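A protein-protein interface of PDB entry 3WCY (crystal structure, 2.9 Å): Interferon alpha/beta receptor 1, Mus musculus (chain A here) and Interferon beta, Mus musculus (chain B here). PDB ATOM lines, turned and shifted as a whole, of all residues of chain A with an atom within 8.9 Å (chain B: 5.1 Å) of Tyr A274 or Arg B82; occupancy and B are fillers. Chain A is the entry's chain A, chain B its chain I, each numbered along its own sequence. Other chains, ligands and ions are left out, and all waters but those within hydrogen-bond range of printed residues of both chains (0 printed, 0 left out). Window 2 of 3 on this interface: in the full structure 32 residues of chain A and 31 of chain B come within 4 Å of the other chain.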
ATOM      1  N   TYR A 218      -5.784   8.404  30.086  1.00  0.00           N
ATOM      2  CA  TYR A 218      -6.355   7.931  31.349  1.00  0.00           C
ATOM      3  C   TYR A 218      -6.507   9.076  32.342  1.00  0.00           C
ATOM      4  O   TYR A 218      -5.612   9.913  32.454  1.00  0.00           O
ATOM      5  CB  TYR A 218      -5.472   6.850  31.997  1.00  0.00           C
ATOM      6  CG  TYR A 218      -5.118   5.667  31.124  1.00  0.00           C
ATOM      7  CD1 TYR A 218      -3.902   5.614  30.450  1.00  0.00           C
ATOM      8  CD2 TYR A 218      -5.947   4.551  31.060  1.00  0.00           C
ATOM      9  CE1 TYR A 218      -3.551   4.509  29.678  1.00  0.00           C
ATOM     10  CE2 TYR A 218      -5.608   3.442  30.287  1.00  0.00           C
ATOM     11  CZ  TYR A 218      -4.405   3.423  29.599  1.00  0.00           C
ATOM     12  OH  TYR A 218      -4.053   2.331  28.842  1.00  0.00           O
ATOM     13  N   TRP A 236       3.586   3.115  38.371  1.00  0.00           N
ATOM     14  CA  TRP A 236       2.786   2.077  37.723  1.00  0.00           C
ATOM     15  C   TRP A 236       3.544   0.765  37.627  1.00  0.00           C
ATOM     16  O   TRP A 236       4.762   0.759  37.457  1.00  0.00           O
ATOM     17  CB  TRP A 236       2.252   2.532  36.347  1.00  0.00           C
ATOM     18  CG  TRP A 236       3.248   2.449  35.226  1.00  0.00           C
ATOM     19  CD1 TRP A 236       4.195   3.372  34.906  1.00  0.00           C
ATOM     20  CD2 TRP A 236       3.385   1.385  34.275  1.00  0.00           C
ATOM     21  NE1 TRP A 236       4.911   2.955  33.811  1.00  0.00           N
ATOM     22  CE2 TRP A 236       4.446   1.729  33.412  1.00  0.00           C
ATOM     23  CE3 TRP A 236       2.718   0.165  34.071  1.00  0.00           C
ATOM     24  CZ2 TRP A 236       4.862   0.896  32.366  1.00  0.00           C
ATOM     25  CZ3 TRP A 236       3.126  -0.655  33.031  1.00  0.00           C
ATOM     26  CH2 TRP A 236       4.187  -0.289  32.194  1.00  0.00           C
ATOM     27  N   LEU A 237       2.824  -0.345  37.732  1.00  0.00           N
ATOM     28  CA  LEU A 237       3.432  -1.668  37.658  1.00  0.00           C
ATOM     29  C   LEU A 237       2.588  -2.533  36.727  1.00  0.00           C
ATOM     30  O   LEU A 237       1.369  -2.523  36.867  1.00  0.00           O
ATOM     31  CB  LEU A 237       3.522  -2.278  39.075  1.00  0.00           C
ATOM     32  CG  LEU A 237       4.428  -3.495  39.276  1.00  0.00           C
ATOM     33  CD1 LEU A 237       5.886  -3.106  39.324  1.00  0.00           C
ATOM     34  CD2 LEU A 237       4.058  -4.243  40.545  1.00  0.00           C
ATOM     35  N   PRO A 238       3.192  -3.255  35.756  1.00  0.00           N
ATOM     36  CA  PRO A 238       2.380  -4.104  34.863  1.00  0.00           C
ATOM     37  C   PRO A 238       1.698  -5.255  35.608  1.00  0.00           C
ATOM     38  O   PRO A 238       2.293  -5.819  36.530  1.00  0.00           O
ATOM     39  CB  PRO A 238       3.392  -4.614  33.836  1.00  0.00           C
ATOM     40  CG  PRO A 238       4.709  -4.499  34.493  1.00  0.00           C
ATOM     41  CD  PRO A 238       4.633  -3.358  35.448  1.00  0.00           C
ATOM     42  N   GLY A 239       0.460  -5.562  35.207  1.00  0.00           N
ATOM     43  CA  GLY A 239      -0.415  -6.584  35.793  1.00  0.00           C
ATOM     44  C   GLY A 239       0.195  -7.902  36.246  1.00  0.00           C
ATOM     45  O   GLY A 239      -0.111  -8.381  37.345  1.00  0.00           O
ATOM     46  N   TYR A 240       1.063  -8.487  35.403  1.00  0.00           N
ATOM     47  CA  TYR A 240       1.725  -9.770  35.645  1.00  0.00           C
ATOM     48  C   TYR A 240       2.798  -9.741  36.729  1.00  0.00           C
ATOM     49  O   TYR A 240       3.178 -10.808  37.203  1.00  0.00           O
ATOM     50  CB  TYR A 240       2.303 -10.343  34.328  1.00  0.00           C
ATOM     51  CG  TYR A 240       3.650  -9.778  33.926  1.00  0.00           C
ATOM     52  CD1 TYR A 240       4.834 -10.380  34.344  1.00  0.00           C
ATOM     53  CD2 TYR A 240       3.743  -8.643  33.121  1.00  0.00           C
ATOM     54  CE1 TYR A 240       6.077  -9.858  33.992  1.00  0.00           C
ATOM     55  CE2 TYR A 240       4.983  -8.113  32.758  1.00  0.00           C
ATOM     56  CZ  TYR A 240       6.149  -8.728  33.193  1.00  0.00           C
ATOM     57  OH  TYR A 240       7.384  -8.228  32.841  1.00  0.00           O
ATOM     58  N   LYS A 253       7.558   1.118  37.976  1.00  0.00           N
ATOM     59  CA  LYS A 253       7.906   2.040  36.888  1.00  0.00           C
ATOM     60  C   LYS A 253       7.361   3.454  37.190  1.00  0.00           C
ATOM     61  O   LYS A 253       6.286   3.563  37.786  1.00  0.00           O
ATOM     62  CB  LYS A 253       7.384   1.504  35.542  1.00  0.00           C
ATOM     63  N   PRO A 254       8.083   4.549  36.833  1.00  0.00           N
ATOM     64  CA  PRO A 254       7.589   5.892  37.181  1.00  0.00           C
ATOM     65  C   PRO A 254       6.618   6.516  36.188  1.00  0.00           C
ATOM     66  O   PRO A 254       6.444   6.009  35.084  1.00  0.00           O
ATOM     67  CB  PRO A 254       8.874   6.709  37.315  1.00  0.00           C
ATOM     68  CG  PRO A 254       9.868   6.014  36.438  1.00  0.00           C
ATOM     69  CD  PRO A 254       9.390   4.624  36.147  1.00  0.00           C
ATOM     70  N   PHE A 268      -2.483  10.687  32.254  1.00  0.00           N
ATOM     71  CA  PHE A 268      -1.348   9.969  31.664  1.00  0.00           C
ATOM     72  C   PHE A 268      -1.740   9.222  30.379  1.00  0.00           C
ATOM     73  O   PHE A 268      -2.867   8.733  30.280  1.00  0.00           O
ATOM     74  CB  PHE A 268      -0.677   9.040  32.700  1.00  0.00           C
ATOM     75  CG  PHE A 268      -1.586   8.126  33.496  1.00  0.00           C
ATOM     76  CD1 PHE A 268      -1.751   6.795  33.135  1.00  0.00           C
ATOM     77  CD2 PHE A 268      -2.236   8.583  34.638  1.00  0.00           C
ATOM     78  CE1 PHE A 268      -2.567   5.943  33.885  1.00  0.00           C
ATOM     79  CE2 PHE A 268      -3.064   7.733  35.381  1.00  0.00           C
ATOM     80  CZ  PHE A 268      -3.227   6.421  34.995  1.00  0.00           C
ATOM     81  N   SER A 269      -0.825   9.161  29.387  1.00  0.00           N
ATOM     82  CA  SER A 269      -1.084   8.493  28.100  1.00  0.00           C
ATOM     83  C   SER A 269      -0.527   7.063  28.001  1.00  0.00           C
ATOM     84  O   SER A 269       0.425   6.715  28.704  1.00  0.00           O
ATOM     85  CB  SER A 269      -0.617   9.350  26.924  1.00  0.00           C
ATOM     86  OG  SER A 269       0.744   9.136  26.582  1.00  0.00           O
ATOM     87  N   GLN A 270      -1.112   6.261  27.086  1.00  0.00           N
ATOM     88  CA  GLN A 270      -0.792   4.855  26.800  1.00  0.00           C
ATOM     89  C   GLN A 270       0.676   4.568  26.408  1.00  0.00           C
ATOM     90  O   GLN A 270       1.100   3.409  26.464  1.00  0.00           O
ATOM     91  CB  GLN A 270      -1.748   4.288  25.730  1.00  0.00           C
ATOM     92  CG  GLN A 270      -3.213   4.197  26.161  1.00  0.00           C
ATOM     93  CD  GLN A 270      -4.087   3.391  25.219  1.00  0.00           C
ATOM     94  OE1 GLN A 270      -3.933   3.416  23.989  1.00  0.00           O
ATOM     95  NE2 GLN A 270      -5.064   2.692  25.780  1.00  0.00           N
ATOM     96  N   ASP A 271       1.439   5.601  25.994  1.00  0.00           N
ATOM     97  CA  ASP A 271       2.845   5.466  25.591  1.00  0.00           C
ATOM     98  C   ASP A 271       3.742   5.101  26.773  1.00  0.00           C
ATOM     99  O   ASP A 271       4.635   4.265  26.639  1.00  0.00           O
ATOM    100  CB  ASP A 271       3.343   6.761  24.927  1.00  0.00           C
ATOM    101  CG  ASP A 271       2.449   7.251  23.812  1.00  0.00           C
ATOM    102  OD1 ASP A 271       2.859   7.150  22.637  1.00  0.00           O
ATOM    103  OD2 ASP A 271       1.328   7.721  24.115  1.00  0.00           O
ATOM    104  N   THR A 272       3.484   5.736  27.926  1.00  0.00           N
ATOM    105  CA  THR A 272       4.209   5.578  29.185  1.00  0.00           C
ATOM    106  C   THR A 272       3.780   4.309  29.938  1.00  0.00           C
ATOM    107  O   THR A 272       4.631   3.535  30.382  1.00  0.00           O
ATOM    108  CB  THR A 272       4.085   6.871  30.024  1.00  0.00           C
ATOM    109  OG1 THR A 272       2.755   7.394  29.913  1.00  0.00           O
ATOM    110  CG2 THR A 272       5.090   7.945  29.602  1.00  0.00           C
ATOM    111  N   VAL A 273       2.457   4.101  30.054  1.00  0.00           N
ATOM    112  CA  VAL A 273       1.810   2.961  30.711  1.00  0.00           C
ATOM    113  C   VAL A 273       1.352   1.973  29.614  1.00  0.00           C
ATOM    114  O   VAL A 273       0.159   1.835  29.306  1.00  0.00           O
ATOM    115  CB  VAL A 273       0.679   3.421  31.677  1.00  0.00           C
ATOM    116  CG1 VAL A 273       1.259   4.047  32.937  1.00  0.00           C
ATOM    117  CG2 VAL A 273      -0.277   4.401  31.003  1.00  0.00           C
ATOM    118  N   TYR A 274       2.342   1.306  29.008  1.00  0.00           N
ATOM    119  CA  TYR A 274       2.153   0.431  27.860  1.00  0.00           C
ATOM    120  C   TYR A 274       1.422  -0.900  27.993  1.00  0.00           C
ATOM    121  O   TYR A 274       0.894  -1.369  26.982  1.00  0.00           O
ATOM    122  CB  TYR A 274       3.424   0.311  27.023  1.00  0.00           C
ATOM    123  CG  TYR A 274       4.646  -0.182  27.761  1.00  0.00           C
ATOM    124  CD1 TYR A 274       4.949  -1.539  27.813  1.00  0.00           C
ATOM    125  CD2 TYR A 274       5.571   0.714  28.292  1.00  0.00           C
ATOM    126  CE1 TYR A 274       6.114  -1.996  28.423  1.00  0.00           C
ATOM    127  CE2 TYR A 274       6.741   0.269  28.905  1.00  0.00           C
ATOM    128  CZ  TYR A 274       7.011  -1.090  28.966  1.00  0.00           C
ATOM    129  OH  TYR A 274       8.152  -1.551  29.580  1.00  0.00           O
ATOM    130  N   THR A 275       1.363  -1.504  29.189  1.00  0.00           N
ATOM    131  CA  THR A 275       0.664  -2.789  29.351  1.00  0.00           C
ATOM    132  C   THR A 275      -0.856  -2.663  29.342  1.00  0.00           C
ATOM    133  O   THR A 275      -1.390  -1.596  29.638  1.00  0.00           O
ATOM    134  CB  THR A 275       1.222  -3.623  30.517  1.00  0.00           C
ATOM    135  OG1 THR A 275       1.205  -2.855  31.722  1.00  0.00           O
ATOM    136  CG2 THR A 275       2.616  -4.167  30.232  1.00  0.00           C
ATOM    137  N   GLY A 276      -1.528  -3.755  28.976  1.00  0.00           N
ATOM    138  CA  GLY A 276      -2.986  -3.840  28.906  1.00  0.00           C
ATOM    139  C   GLY A 276      -3.648  -3.780  30.265  1.00  0.00           C
ATOM    140  O   GLY A 276      -4.781  -3.304  30.398  1.00  0.00           O
ATOM    141  N   THR A 277      -2.933  -4.292  31.276  1.00  0.00           N
ATOM    142  CA  THR A 277      -3.339  -4.289  32.671  1.00  0.00           C
ATOM    143  C   THR A 277      -2.186  -3.759  33.494  1.00  0.00           C
ATOM    144  O   THR A 277      -1.030  -4.102  33.235  1.00  0.00           O
ATOM    145  CB  THR A 277      -3.795  -5.676  33.150  1.00  0.00           C
ATOM    146  OG1 THR A 277      -2.826  -6.671  32.828  1.00  0.00           O
ATOM    147  CG2 THR A 277      -5.151  -6.066  32.617  1.00  0.00           C
ATOM    148  N   PHE A 278      -2.496  -2.895  34.470  1.00  0.00           N
ATOM    149  CA  PHE A 278      -1.501  -2.310  35.361  1.00  0.00           C
ATOM    150  C   PHE A 278      -2.041  -1.848  36.723  1.00  0.00           C
ATOM    151  O   PHE A 278      -3.250  -1.674  36.893  1.00  0.00           O
ATOM    152  CB  PHE A 278      -0.621  -1.248  34.652  1.00  0.00           C
ATOM    153  CG  PHE A 278      -1.281   0.021  34.167  1.00  0.00           C
ATOM    154  CD1 PHE A 278      -1.163   1.204  34.890  1.00  0.00           C
ATOM    155  CD2 PHE A 278      -1.936   0.060  32.943  1.00  0.00           C
ATOM    156  CE1 PHE A 278      -1.742   2.392  34.424  1.00  0.00           C
ATOM    157  CE2 PHE A 278      -2.512   1.247  32.477  1.00  0.00           C
ATOM    158  CZ  PHE A 278      -2.413   2.404  33.221  1.00  0.00           C
ATOM    159  N   SER A 301      -7.149  -1.892  30.910  1.00  0.00           N
ATOM    160  CA  SER A 301      -7.440  -1.017  29.776  1.00  0.00           C
ATOM    161  C   SER A 301      -7.726  -1.878  28.548  1.00  0.00           C
ATOM    162  O   SER A 301      -6.802  -2.352  27.882  1.00  0.00           O
ATOM    163  CB  SER A 301      -6.295  -0.039  29.530  1.00  0.00           C
ATOM    164  OG  SER A 301      -5.058  -0.698  29.309  1.00  0.00           O
ATOM    165  N   LEU B  20       1.932  -9.547  18.885  1.00  0.00           N
ATOM    166  CA  LEU B  20       2.955  -9.120  19.840  1.00  0.00           C
ATOM    167  C   LEU B  20       4.264  -9.882  19.657  1.00  0.00           C
ATOM    168  O   LEU B  20       5.321  -9.261  19.714  1.00  0.00           O
ATOM    169  CB  LEU B  20       2.459  -9.246  21.289  1.00  0.00           C
ATOM    170  CG  LEU B  20       1.642  -8.078  21.835  1.00  0.00           C
ATOM    171  CD1 LEU B  20       0.968  -8.445  23.149  1.00  0.00           C
ATOM    172  CD2 LEU B  20       2.502  -6.827  22.017  1.00  0.00           C
ATOM    173  N   GLU B  77      12.253  -4.673  24.874  1.00  0.00           N
ATOM    174  CA  GLU B  77      11.756  -5.047  26.205  1.00  0.00           C
ATOM    175  C   GLU B  77      10.278  -4.687  26.377  1.00  0.00           C
ATOM    176  O   GLU B  77       9.503  -5.519  26.843  1.00  0.00           O
ATOM    177  CB  GLU B  77      12.639  -4.484  27.351  1.00  0.00           C
ATOM    178  CG  GLU B  77      12.720  -2.968  27.466  1.00  0.00           C
ATOM    179  CD  GLU B  77      12.583  -2.435  28.881  1.00  0.00           C
ATOM    180  OE1 GLU B  77      13.528  -2.619  29.681  1.00  0.00           O
ATOM    181  OE2 GLU B  77      11.535  -1.821  29.186  1.00  0.00           O
ATOM    182  N   THR B  78       9.890  -3.484  25.898  1.00  0.00           N
ATOM    183  CA  THR B  78       8.546  -2.910  25.906  1.00  0.00           C
ATOM    184  C   THR B  78       7.513  -3.893  25.352  1.00  0.00           C
ATOM    185  O   THR B  78       6.442  -4.053  25.939  1.00  0.00           O
ATOM    186  CB  THR B  78       8.582  -1.572  25.156  1.00  0.00           C
ATOM    187  OG1 THR B  78       9.457  -0.694  25.860  1.00  0.00           O
ATOM    188  CG2 THR B  78       7.206  -0.924  25.001  1.00  0.00           C
ATOM    189  N   ILE B  79       7.853  -4.564  24.247  1.00  0.00           N
ATOM    190  CA  ILE B  79       6.987  -5.548  23.604  1.00  0.00           C
ATOM    191  C   ILE B  79       6.907  -6.866  24.408  1.00  0.00           C
ATOM    192  O   ILE B  79       5.828  -7.438  24.511  1.00  0.00           O
ATOM    193  CB  ILE B  79       7.326  -5.678  22.080  1.00  0.00           C
ATOM    194  CG1 ILE B  79       6.210  -5.087  21.196  1.00  0.00           C
ATOM    195  CG2 ILE B  79       7.689  -7.086  21.643  1.00  0.00           C
ATOM    196  CD1 ILE B  79       6.308  -3.605  20.956  1.00  0.00           C
ATOM    197  N   VAL B  80       8.029  -7.307  25.016  1.00  0.00           N
ATOM    198  CA  VAL B  80       8.083  -8.527  25.836  1.00  0.00           C
ATOM    199  C   VAL B  80       7.311  -8.316  27.143  1.00  0.00           C
ATOM    200  O   VAL B  80       6.628  -9.234  27.602  1.00  0.00           O
ATOM    201  CB  VAL B  80       9.522  -9.063  26.066  1.00  0.00           C
ATOM    202  CG1 VAL B  80       9.499 -10.448  26.716  1.00  0.00           C
ATOM    203  CG2 VAL B  80      10.312  -9.110  24.755  1.00  0.00           C
ATOM    204  N   VAL B  81       7.379  -7.097  27.712  1.00  0.00           N
ATOM    205  CA  VAL B  81       6.621  -6.722  28.909  1.00  0.00           C
ATOM    206  C   VAL B  81       5.131  -6.794  28.515  1.00  0.00           C
ATOM    207  O   VAL B  81       4.350  -7.448  29.210  1.00  0.00           O
ATOM    208  CB  VAL B  81       7.030  -5.325  29.461  1.00  0.00           C
ATOM    209  CG1 VAL B  81       6.174  -4.921  30.663  1.00  0.00           C
ATOM    210  CG2 VAL B  81       8.511  -5.279  29.826  1.00  0.00           C
ATOM    211  N   ARG B  82       4.780  -6.201  27.343  1.00  0.00           N
ATOM    212  CA  ARG B  82       3.433  -6.180  26.750  1.00  0.00           C
ATOM    213  C   ARG B  82       2.869  -7.581  26.509  1.00  0.00           C
ATOM    214  O   ARG B  82       1.708  -7.810  26.848  1.00  0.00           O
ATOM    215  CB  ARG B  82       3.422  -5.377  25.439  1.00  0.00           C
ATOM    216  CG  ARG B  82       2.893  -3.961  25.588  1.00  0.00           C
ATOM    217  CD  ARG B  82       1.895  -3.625  24.498  1.00  0.00           C
ATOM    218  NE  ARG B  82       2.551  -3.394  23.211  1.00  0.00           N
ATOM    219  CZ  ARG B  82       1.912  -3.284  22.051  1.00  0.00           C
ATOM    220  NH1 ARG B  82       2.591  -3.074  20.932  1.00  0.00           N
ATOM    221  NH2 ARG B  82       0.590  -3.395  22.000  1.00  0.00           N
ATOM    222  N   LEU B  83       3.696  -8.506  25.937  1.00  0.00           N
ATOM    223  CA  LEU B  83       3.364  -9.904  25.629  1.00  0.00           C
ATOM    224  C   LEU B  83       3.051 -10.691  26.902  1.00  0.00           C
ATOM    225  O   LEU B  83       1.948 -11.230  27.009  1.00  0.00           O
ATOM    226  CB  LEU B  83       4.483 -10.583  24.791  1.00  0.00           C
ATOM    227  CG  LEU B  83       4.447 -12.135  24.608  1.00  0.00           C
ATOM    228  CD1 LEU B  83       3.222 -12.611  23.806  1.00  0.00           C
ATOM    229  CD2 LEU B  83       5.709 -12.631  23.930  1.00  0.00           C
ATOM    230  N   LEU B  84       3.999 -10.715  27.881  1.00  0.00           N
ATOM    231  CA  LEU B  84       3.827 -11.401  29.167  1.00  0.00           C
ATOM    232  C   LEU B  84       2.525 -10.967  29.821  1.00  0.00           C
ATOM    233  O   LEU B  84       1.818 -11.801  30.373  1.00  0.00           O
ATOM    234  CB  LEU B  84       4.990 -11.119  30.140  1.00  0.00           C
ATOM    235  CG  LEU B  84       6.344 -11.778  29.886  1.00  0.00           C
ATOM    236  CD1 LEU B  84       7.427 -11.085  30.685  1.00  0.00           C
ATOM    237  CD2 LEU B  84       6.324 -13.240  30.268  1.00  0.00           C
ATOM    238  N   ASP B  85       2.192  -9.676  29.728  1.00  0.00           N
ATOM    239  CA  ASP B  85       0.973  -9.154  30.318  1.00  0.00           C
ATOM    240  C   ASP B  85      -0.287  -9.631  29.611  1.00  0.00           C
ATOM    241  O   ASP B  85      -1.233 -10.009  30.299  1.00  0.00           O
ATOM    242  CB  ASP B  85       1.006  -7.629  30.441  1.00  0.00           C
ATOM    243  CG  ASP B  85      -0.130  -7.100  31.284  1.00  0.00           C
ATOM    244  OD1 ASP B  85      -0.047  -7.214  32.526  1.00  0.00           O
ATOM    245  OD2 ASP B  85      -1.140  -6.653  30.702  1.00  0.00           O
ATOM    246  N   GLU B  86      -0.309  -9.632  28.265  1.00  0.00           N
ATOM    247  CA  GLU B  86      -1.479 -10.101  27.513  1.00  0.00           C
ATOM    248  C   GLU B  86      -1.633 -11.626  27.688  1.00  0.00           C
ATOM    249  O   GLU B  86      -2.764 -12.116  27.780  1.00  0.00           O
ATOM    250  CB  GLU B  86      -1.420  -9.659  26.032  1.00  0.00           C
ATOM    251  CG  GLU B  86      -2.691  -9.888  25.226  1.00  0.00           C
ATOM    252  CD  GLU B  86      -3.894  -9.038  25.596  1.00  0.00           C
ATOM    253  OE1 GLU B  86      -3.913  -7.839  25.237  1.00  0.00           O
ATOM    254  OE2 GLU B  86      -4.841  -9.588  26.201  1.00  0.00           O
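Printed residues of chain B within 4 Å of Gly A239: Asp B85.
Of the printed residues of chain B, Tyr A240 touches Val B81 (3.7 Å), Leu B84 (3.6 Å) and Asp B85 (3.3 Å).
Of chain B, only Glu B77, Thr B78, Val B81 and Arg B82 come within 4 Å of Tyr A274.
Printed residues of chain B within 4 Å of Thr A275: Val B81 and Asp B85.
Of the printed residues of chain B, Thr A277 touches Asp B85 (2.7 Å).
Of chain A, only Tyr A274 comes within 4 Å of Thr B78.
Ile B79 touches none of the printed residues of chain A.
Val B81 touches three residues of chain A.
Arg B82 touches one residue of chain A.
Printed residues of chain A within 4 Å of Leu B84: Tyr A240 (3.6 Å).
The nearest residue of chain A that does not touch Arg B82 is Thr A275 (4.1 Å).
The nearest printed residue of chain B that does not touch Thr A275 is Arg B82 (4.1 Å).
Hydrophobic or aromatic side chains of chain A within 4 Å of the printed part of chain B: Tyr A240 and Tyr A274.
Along chain A the printed residues that touch a printed residue of chain B span positions 239 to 277.
Among the printed residues, 12 pairs touch across the chains.
CE2 of Tyr A240 touches O of Val B81 (3.7 Å).
CD1 of Leu B84 touches OH of Tyr A240 (3.6 Å).
Thr B78 touches Tyr A274 (O to CE1, 3.2 Å).
Tyr A274 touches Val B81 (CE1 to CB, 3.6 Å).
Arg B82 touches Tyr A274 (CD to O, 3.5 Å).
Thr A275 touches Val B81.
CG of Asp B85 touches CB of Thr A275 (3.8 Å).
The backbone NH of Gly A276 lies within hydrogen-bond range of the side-chain carboxylate of Asp B85 (3.4 Å).
OH of Tyr A274 lies within hydrogen-bond range of OE2 of Glu B77, at 3.4 Å.
The backbone NH of Tyr A240 sits at hydrogen-bond distance from the side-chain carboxylate of Asp B85 (3.3 Å).
The side-chain carboxylate (OD2) of Asp B85 lies within hydrogen-bond range of the side-chain hydroxyl (OG1) of Thr A277 (2.7 Å).
The backbone NH (N) of Gly A239 is in hydrogen-bond range of the side-chain carboxylate (OD1) of Asp B85 (3.2 Å).
The backbone carbonyl oxygen (O) of Gly A276 lies within hydrogen-bond range of the backbone NH (N) of Ser A301 (2.8 Å).
The backbone NH (N) of Gly A239 is in hydrogen-bond range of the backbone carbonyl oxygen (O) of Thr A277.
O of Thr A277 sits at hydrogen-bond distance from OG1 of Thr A275 (3.0 Å).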
